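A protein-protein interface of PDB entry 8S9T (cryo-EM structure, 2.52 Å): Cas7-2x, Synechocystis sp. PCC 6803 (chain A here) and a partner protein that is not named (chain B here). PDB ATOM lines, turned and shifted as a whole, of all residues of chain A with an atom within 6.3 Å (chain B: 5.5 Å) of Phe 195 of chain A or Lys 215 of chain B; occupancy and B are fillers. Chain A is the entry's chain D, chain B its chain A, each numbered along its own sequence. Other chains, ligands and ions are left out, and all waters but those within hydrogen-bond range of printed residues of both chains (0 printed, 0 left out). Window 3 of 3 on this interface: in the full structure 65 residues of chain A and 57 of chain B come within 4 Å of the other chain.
OE1 of Gln 212 of chain B is in hydrogen-bond range of NZ of Lys 215 of chain B. O of Leu 199 of chain A lies within hydrogen-bond range of NE2 of Gln 201 of chain A, 3.0 Å away.
Phe 195 of chain A touches three residues of chain B. Of the printed residues of chain A, Lys 215 of chain B touches Phe 195 (3.6 Å) and Leu 199 (3.7 Å). Of the printed residues of chain A, Leu 59 of chain B touches Ile 194 and Phe 195. Of the printed residues of chain B, Pro 191 of chain A touches Tyr 218. Of the printed residues of chain A, Ile 211 of chain B touches Leu 198 (3.97 Å) and Leu 199 (3.9 Å). Printed residues of chain B within 4 Å of Leu 199 of chain A: Ile 211 (3.9 Å), Gln 212 (3.8 Å) and Lys 215 (3.7 Å). Printed residues of chain B within 4 Å of Leu 198 of chain A: Ser 180 and Ile 211. Glu 192 of chain A touches none of the printed residues of chain B.
Among the printed residues, merely in contact across the chains: Pro 191 of chain A with Tyr 218 of chain B, Ile 194 of chain A with Leu 59 of chain B, Phe 195 of chain A with Leu 59 of chain B, Phe 195 of chain A with Lys 215 of chain B, Phe 195 of chain A with Tyr 218 of chain B, Leu 198 of chain A with Ser 180 of chain B, Leu 198 of chain A with Ile 211 of chain B, Leu 199 of chain A with Ile 211 of chain B, Leu 199 of chain A with Gln 212 of chain B and Leu 199 of chain A with Lys 215 of chain B.
Printed residues of chain A that touch a printed residue of chain B: Pro 191, Ile 194, Phe 195, Leu 198 and Leu 199. Hydrophobic or aromatic side chains of chain A that line the printed part of chain B: Pro 191, Ile 194, Phe 195, Leu 198 and Leu 199. Of the 10 printed residues of chain B, 6 touch a printed residue of chain A. Among the printed residues, 10 pairs touch across the chains. Among the printed residues, no Asp or Glu carboxylate lies within 4 Å of a Lys or Arg side-chain nitrogen of the other chain.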
ATOM      1  N   LYS A 190     -29.656 -12.786  20.500  1.00  0.00           N
ATOM      2  CA  LYS A 190     -28.873 -11.703  19.930  1.00  0.00           C
ATOM      3  C   LYS A 190     -28.126 -12.169  18.694  1.00  0.00           C
ATOM      4  O   LYS A 190     -27.811 -13.352  18.561  1.00  0.00           O
ATOM      5  CB  LYS A 190     -27.855 -11.169  20.944  1.00  0.00           C
ATOM      6  CG  LYS A 190     -28.446 -10.598  22.195  1.00  0.00           C
ATOM      7  CD  LYS A 190     -27.357 -10.103  23.105  1.00  0.00           C
ATOM      8  CE  LYS A 190     -27.927  -9.621  24.416  1.00  0.00           C
ATOM      9  NZ  LYS A 190     -28.650  -8.333  24.257  1.00  0.00           N
ATOM     10  N   PRO A 191     -27.827 -11.249  17.775  1.00  0.00           N
ATOM     11  CA  PRO A 191     -27.116 -11.639  16.552  1.00  0.00           C
ATOM     12  C   PRO A 191     -25.739 -12.201  16.806  1.00  0.00           C
ATOM     13  O   PRO A 191     -25.327 -13.153  16.140  1.00  0.00           O
ATOM     14  CB  PRO A 191     -27.056 -10.330  15.764  1.00  0.00           C
ATOM     15  CG  PRO A 191     -28.208  -9.545  16.257  1.00  0.00           C
ATOM     16  CD  PRO A 191     -28.287  -9.854  17.712  1.00  0.00           C
ATOM     17  N   GLU A 192     -25.002 -11.630  17.755  1.00  0.00           N
ATOM     18  CA  GLU A 192     -23.662 -12.125  18.025  1.00  0.00           C
ATOM     19  C   GLU A 192     -23.698 -13.546  18.548  1.00  0.00           C
ATOM     20  O   GLU A 192     -22.789 -14.332  18.270  1.00  0.00           O
ATOM     21  CB  GLU A 192     -22.956 -11.218  19.028  1.00  0.00           C
ATOM     22  CG  GLU A 192     -22.801  -9.786  18.568  1.00  0.00           C
ATOM     23  CD  GLU A 192     -24.060  -8.962  18.754  1.00  0.00           C
ATOM     24  OE1 GLU A 192     -24.077  -7.800  18.302  1.00  0.00           O
ATOM     25  OE2 GLU A 192     -25.021  -9.468  19.368  1.00  0.00           O
ATOM     26  N   GLY A 193     -24.723 -13.884  19.327  1.00  0.00           N
ATOM     27  CA  GLY A 193     -24.842 -15.227  19.853  1.00  0.00           C
ATOM     28  C   GLY A 193     -25.386 -16.242  18.878  1.00  0.00           C
ATOM     29  O   GLY A 193     -25.041 -17.421  18.957  1.00  0.00           O
ATOM     30  N   ILE A 194     -26.260 -15.823  17.969  1.00  0.00           N
ATOM     31  CA  ILE A 194     -26.698 -16.749  16.933  1.00  0.00           C
ATOM     32  C   ILE A 194     -25.558 -17.057  15.964  1.00  0.00           C
ATOM     33  O   ILE A 194     -25.348 -18.215  15.594  1.00  0.00           O
ATOM     34  CB  ILE A 194     -27.972 -16.236  16.231  1.00  0.00           C
ATOM     35  CG1 ILE A 194     -28.565 -17.350  15.395  1.00  0.00           C
ATOM     36  CG2 ILE A 194     -27.698 -15.082  15.327  1.00  0.00           C
ATOM     37  CD1 ILE A 194     -29.264 -18.395  16.229  1.00  0.00           C
ATOM     38  N   PHE A 195     -24.811 -16.045  15.530  1.00  0.00           N
ATOM     39  CA  PHE A 195     -23.675 -16.316  14.659  1.00  0.00           C
ATOM     40  C   PHE A 195     -22.566 -17.045  15.394  1.00  0.00           C
ATOM     41  O   PHE A 195     -21.831 -17.825  14.785  1.00  0.00           O
ATOM     42  CB  PHE A 195     -23.166 -15.024  14.034  1.00  0.00           C
ATOM     43  CG  PHE A 195     -24.126 -14.426  13.065  1.00  0.00           C
ATOM     44  CD1 PHE A 195     -24.569 -15.153  11.985  1.00  0.00           C
ATOM     45  CD2 PHE A 195     -24.590 -13.143  13.234  1.00  0.00           C
ATOM     46  CE1 PHE A 195     -25.464 -14.613  11.105  1.00  0.00           C
ATOM     47  CE2 PHE A 195     -25.479 -12.599  12.355  1.00  0.00           C
ATOM     48  CZ  PHE A 195     -25.919 -13.331  11.288  1.00  0.00           C
ATOM     49  N   SER A 196     -22.418 -16.801  16.692  1.00  0.00           N
ATOM     50  CA  SER A 196     -21.537 -17.633  17.495  1.00  0.00           C
ATOM     51  C   SER A 196     -21.998 -19.079  17.492  1.00  0.00           C
ATOM     52  O   SER A 196     -21.178 -20.000  17.446  1.00  0.00           O
ATOM     53  CB  SER A 196     -21.470 -17.093  18.918  1.00  0.00           C
ATOM     54  OG  SER A 196     -20.585 -17.855  19.708  1.00  0.00           O
ATOM     55  N   ALA A 197     -23.311 -19.297  17.555  1.00  0.00           N
ATOM     56  CA  ALA A 197     -23.849 -20.649  17.503  1.00  0.00           C
ATOM     57  C   ALA A 197     -23.573 -21.306  16.168  1.00  0.00           C
ATOM     58  O   ALA A 197     -23.369 -22.523  16.101  1.00  0.00           O
ATOM     59  CB  ALA A 197     -25.349 -20.623  17.776  1.00  0.00           C
ATOM     60  N   LEU A 198     -23.567 -20.521  15.100  1.00  0.00           N
ATOM     61  CA  LEU A 198     -23.326 -21.047  13.770  1.00  0.00           C
ATOM     62  C   LEU A 198     -21.848 -21.254  13.494  1.00  0.00           C
ATOM     63  O   LEU A 198     -21.495 -22.122  12.695  1.00  0.00           O
ATOM     64  CB  LEU A 198     -23.945 -20.118  12.731  1.00  0.00           C
ATOM     65  CG  LEU A 198     -25.458 -19.983  12.910  1.00  0.00           C
ATOM     66  CD1 LEU A 198     -26.029 -18.877  12.058  1.00  0.00           C
ATOM     67  CD2 LEU A 198     -26.142 -21.287  12.644  1.00  0.00           C
ATOM     68  N   LEU A 199     -20.971 -20.487  14.142  1.00  0.00           N
ATOM     69  CA  LEU A 199     -19.584 -20.420  13.702  1.00  0.00           C
ATOM     70  C   LEU A 199     -18.529 -20.631  14.786  1.00  0.00           C
ATOM     71  O   LEU A 199     -17.484 -21.222  14.508  1.00  0.00           O
ATOM     72  CB  LEU A 199     -19.343 -19.062  13.039  1.00  0.00           C
ATOM     73  CG  LEU A 199     -20.136 -18.757  11.773  1.00  0.00           C
ATOM     74  CD1 LEU A 199     -20.042 -17.296  11.402  1.00  0.00           C
ATOM     75  CD2 LEU A 199     -19.642 -19.625  10.636  1.00  0.00           C
ATOM     76  N   ASP A 200     -18.771 -20.172  16.015  1.00  0.00           N
ATOM     77  CA  ASP A 200     -17.683 -19.827  16.929  1.00  0.00           C
ATOM     78  C   ASP A 200     -17.560 -20.703  18.171  1.00  0.00           C
ATOM     79  O   ASP A 200     -16.690 -20.434  19.003  1.00  0.00           O
ATOM     80  CB  ASP A 200     -17.815 -18.364  17.361  1.00  0.00           C
ATOM     81  CG  ASP A 200     -17.918 -17.418  16.184  1.00  0.00           C
ATOM     82  OD1 ASP A 200     -17.239 -17.658  15.170  1.00  0.00           O
ATOM     83  OD2 ASP A 200     -18.690 -16.442  16.261  1.00  0.00           O
ATOM     84  N   GLN A 201     -18.415 -21.706  18.347  1.00  0.00           N
ATOM     85  CA  GLN A 201     -18.341 -22.671  19.451  1.00  0.00           C
ATOM     86  C   GLN A 201     -18.466 -22.048  20.847  1.00  0.00           C
ATOM     87  O   GLN A 201     -18.141 -22.704  21.839  1.00  0.00           O
ATOM     88  CB  GLN A 201     -17.055 -23.506  19.380  1.00  0.00           C
ATOM     89  CG  GLN A 201     -17.001 -24.524  18.244  1.00  0.00           C
ATOM     90  CD  GLN A 201     -17.094 -23.893  16.864  1.00  0.00           C
ATOM     91  OE1 GLN A 201     -18.019 -24.175  16.100  1.00  0.00           O
ATOM     92  NE2 GLN A 201     -16.130 -23.037  16.538  1.00  0.00           N
ATOM     93  N   LEU B  59     -31.513 -12.564  15.042  1.00  0.00           N
ATOM     94  CA  LEU B  59     -31.328 -11.400  14.189  1.00  0.00           C
ATOM     95  C   LEU B  59     -32.342 -10.309  14.488  1.00  0.00           C
ATOM     96  O   LEU B  59     -32.025  -9.125  14.355  1.00  0.00           O
ATOM     97  CB  LEU B  59     -31.412 -11.806  12.724  1.00  0.00           C
ATOM     98  CG  LEU B  59     -30.416 -12.859  12.273  1.00  0.00           C
ATOM     99  CD1 LEU B  59     -30.538 -13.087  10.795  1.00  0.00           C
ATOM    100  CD2 LEU B  59     -29.016 -12.448  12.651  1.00  0.00           C
ATOM    101  N   SER B 180     -27.779 -20.997   7.320  1.00  0.00           N
ATOM    102  CA  SER B 180     -27.741 -20.764   8.758  1.00  0.00           C
ATOM    103  C   SER B 180     -28.755 -21.615   9.502  1.00  0.00           C
ATOM    104  O   SER B 180     -28.447 -22.159  10.565  1.00  0.00           O
ATOM    105  CB  SER B 180     -27.987 -19.290   9.041  1.00  0.00           C
ATOM    106  OG  SER B 180     -27.018 -18.510   8.382  1.00  0.00           O
ATOM    107  N   ILE B 211     -23.342 -18.487   5.344  1.00  0.00           N
ATOM    108  CA  ILE B 211     -23.498 -18.009   6.710  1.00  0.00           C
ATOM    109  C   ILE B 211     -22.697 -16.736   6.926  1.00  0.00           C
ATOM    110  O   ILE B 211     -23.202 -15.745   7.463  1.00  0.00           O
ATOM    111  CB  ILE B 211     -23.083 -19.112   7.705  1.00  0.00           C
ATOM    112  CG1 ILE B 211     -23.902 -20.380   7.482  1.00  0.00           C
ATOM    113  CG2 ILE B 211     -23.158 -18.632   9.138  1.00  0.00           C
ATOM    114  CD1 ILE B 211     -23.638 -21.470   8.479  1.00  0.00           C
ATOM    115  N   GLN B 212     -21.434 -16.750   6.510  1.00  0.00           N
ATOM    116  CA  GLN B 212     -20.544 -15.622   6.729  1.00  0.00           C
ATOM    117  C   GLN B 212     -21.019 -14.375   6.014  1.00  0.00           C
ATOM    118  O   GLN B 212     -20.863 -13.269   6.532  1.00  0.00           O
ATOM    119  CB  GLN B 212     -19.129 -15.993   6.288  1.00  0.00           C
ATOM    120  CG  GLN B 212     -18.037 -15.006   6.677  1.00  0.00           C
ATOM    121  CD  GLN B 212     -17.796 -14.962   8.162  1.00  0.00           C
ATOM    122  OE1 GLN B 212     -17.825 -13.900   8.777  1.00  0.00           O
ATOM    123  NE2 GLN B 212     -17.590 -16.126   8.756  1.00  0.00           N
ATOM    124  N   TRP B 213     -21.577 -14.523   4.814  1.00  0.00           N
ATOM    125  CA  TRP B 213     -22.121 -13.364   4.115  1.00  0.00           C
ATOM    126  C   TRP B 213     -23.240 -12.683   4.897  1.00  0.00           C
ATOM    127  O   TRP B 213     -23.267 -11.455   5.007  1.00  0.00           O
ATOM    128  CB  TRP B 213     -22.619 -13.775   2.729  1.00  0.00           C
ATOM    129  CG  TRP B 213     -23.092 -12.614   1.934  1.00  0.00           C
ATOM    130  CD1 TRP B 213     -22.363 -11.882   1.057  1.00  0.00           C
ATOM    131  CD2 TRP B 213     -24.396 -12.028   1.958  1.00  0.00           C
ATOM    132  NE1 TRP B 213     -23.123 -10.879   0.535  1.00  0.00           N
ATOM    133  CE2 TRP B 213     -24.375 -10.943   1.078  1.00  0.00           C
ATOM    134  CE3 TRP B 213     -25.572 -12.308   2.655  1.00  0.00           C
ATOM    135  CZ2 TRP B 213     -25.482 -10.149   0.862  1.00  0.00           C
ATOM    136  CZ3 TRP B 213     -26.654 -11.522   2.449  1.00  0.00           C
ATOM    137  CH2 TRP B 213     -26.612 -10.455   1.554  1.00  0.00           C
ATOM    138  N   LEU B 214     -24.156 -13.462   5.470  1.00  0.00           N
ATOM    139  CA  LEU B 214     -25.218 -12.889   6.289  1.00  0.00           C
ATOM    140  C   LEU B 214     -24.670 -12.205   7.536  1.00  0.00           C
ATOM    141  O   LEU B 214     -25.075 -11.090   7.869  1.00  0.00           O
ATOM    142  CB  LEU B 214     -26.232 -13.975   6.649  1.00  0.00           C
ATOM    143  CG  LEU B 214     -27.636 -13.533   7.049  1.00  0.00           C
ATOM    144  CD1 LEU B 214     -28.420 -13.072   5.861  1.00  0.00           C
ATOM    145  CD2 LEU B 214     -28.343 -14.680   7.705  1.00  0.00           C
ATOM    146  N   LYS B 215     -23.765 -12.866   8.255  1.00  0.00           N
ATOM    147  CA  LYS B 215     -23.096 -12.217   9.378  1.00  0.00           C
ATOM    148  C   LYS B 215     -22.442 -10.902   8.960  1.00  0.00           C
ATOM    149  O   LYS B 215     -22.496  -9.911   9.695  1.00  0.00           O
ATOM    150  CB  LYS B 215     -22.078 -13.176   9.994  1.00  0.00           C
ATOM    151  CG  LYS B 215     -21.325 -12.619  11.170  1.00  0.00           C
ATOM    152  CD  LYS B 215     -20.366 -13.653  11.715  1.00  0.00           C
ATOM    153  CE  LYS B 215     -19.201 -13.025  12.445  1.00  0.00           C
ATOM    154  NZ  LYS B 215     -18.257 -12.348  11.512  1.00  0.00           N
ATOM    155  N   ASP B 216     -21.820 -10.873   7.783  1.00  0.00           N
ATOM    156  CA  ASP B 216     -21.239  -9.640   7.270  1.00  0.00           C
ATOM    157  C   ASP B 216     -22.293  -8.617   6.866  1.00  0.00           C
ATOM    158  O   ASP B 216     -22.024  -7.414   6.910  1.00  0.00           O
ATOM    159  CB  ASP B 216     -20.376  -9.937   6.050  1.00  0.00           C
ATOM    160  CG  ASP B 216     -19.135 -10.714   6.384  1.00  0.00           C
ATOM    161  OD1 ASP B 216     -18.690 -10.645   7.545  1.00  0.00           O
ATOM    162  OD2 ASP B 216     -18.612 -11.398   5.480  1.00  0.00           O
ATOM    163  N   ASN B 217     -23.475  -9.060   6.442  1.00  0.00           N
ATOM    164  CA  ASN B 217     -24.416  -8.182   5.759  1.00  0.00           C
ATOM    165  C   ASN B 217     -25.771  -8.013   6.417  1.00  0.00           C
ATOM    166  O   ASN B 217     -26.542  -7.175   5.954  1.00  0.00           O
ATOM    167  CB  ASN B 217     -24.640  -8.654   4.314  1.00  0.00           C
ATOM    168  CG  ASN B 217     -23.436  -8.433   3.447  1.00  0.00           C
ATOM    169  OD1 ASN B 217     -23.328  -7.413   2.780  1.00  0.00           O
ATOM    170  ND2 ASN B 217     -22.501  -9.370   3.480  1.00  0.00           N
ATOM    171  N   TYR B 218     -26.108  -8.800   7.435  1.00  0.00           N
ATOM    172  CA  TYR B 218     -27.487  -8.833   7.914  1.00  0.00           C
ATOM    173  C   TYR B 218     -28.001  -7.457   8.337  1.00  0.00           C
ATOM    174  O   TYR B 218     -29.196  -7.175   8.197  1.00  0.00           O
ATOM    175  CB  TYR B 218     -27.626  -9.825   9.069  1.00  0.00           C
ATOM    176  CG  TYR B 218     -27.241  -9.277  10.404  1.00  0.00           C
ATOM    177  CD1 TYR B 218     -25.916  -9.188  10.781  1.00  0.00           C
ATOM    178  CD2 TYR B 218     -28.208  -8.835  11.287  1.00  0.00           C
ATOM    179  CE1 TYR B 218     -25.568  -8.695  12.002  1.00  0.00           C
ATOM    180  CE2 TYR B 218     -27.867  -8.325  12.498  1.00  0.00           C
ATOM    181  CZ  TYR B 218     -26.545  -8.260  12.856  1.00  0.00           C
ATOM    182  OH  TYR B 218     -26.192  -7.743  14.074  1.00  0.00           O
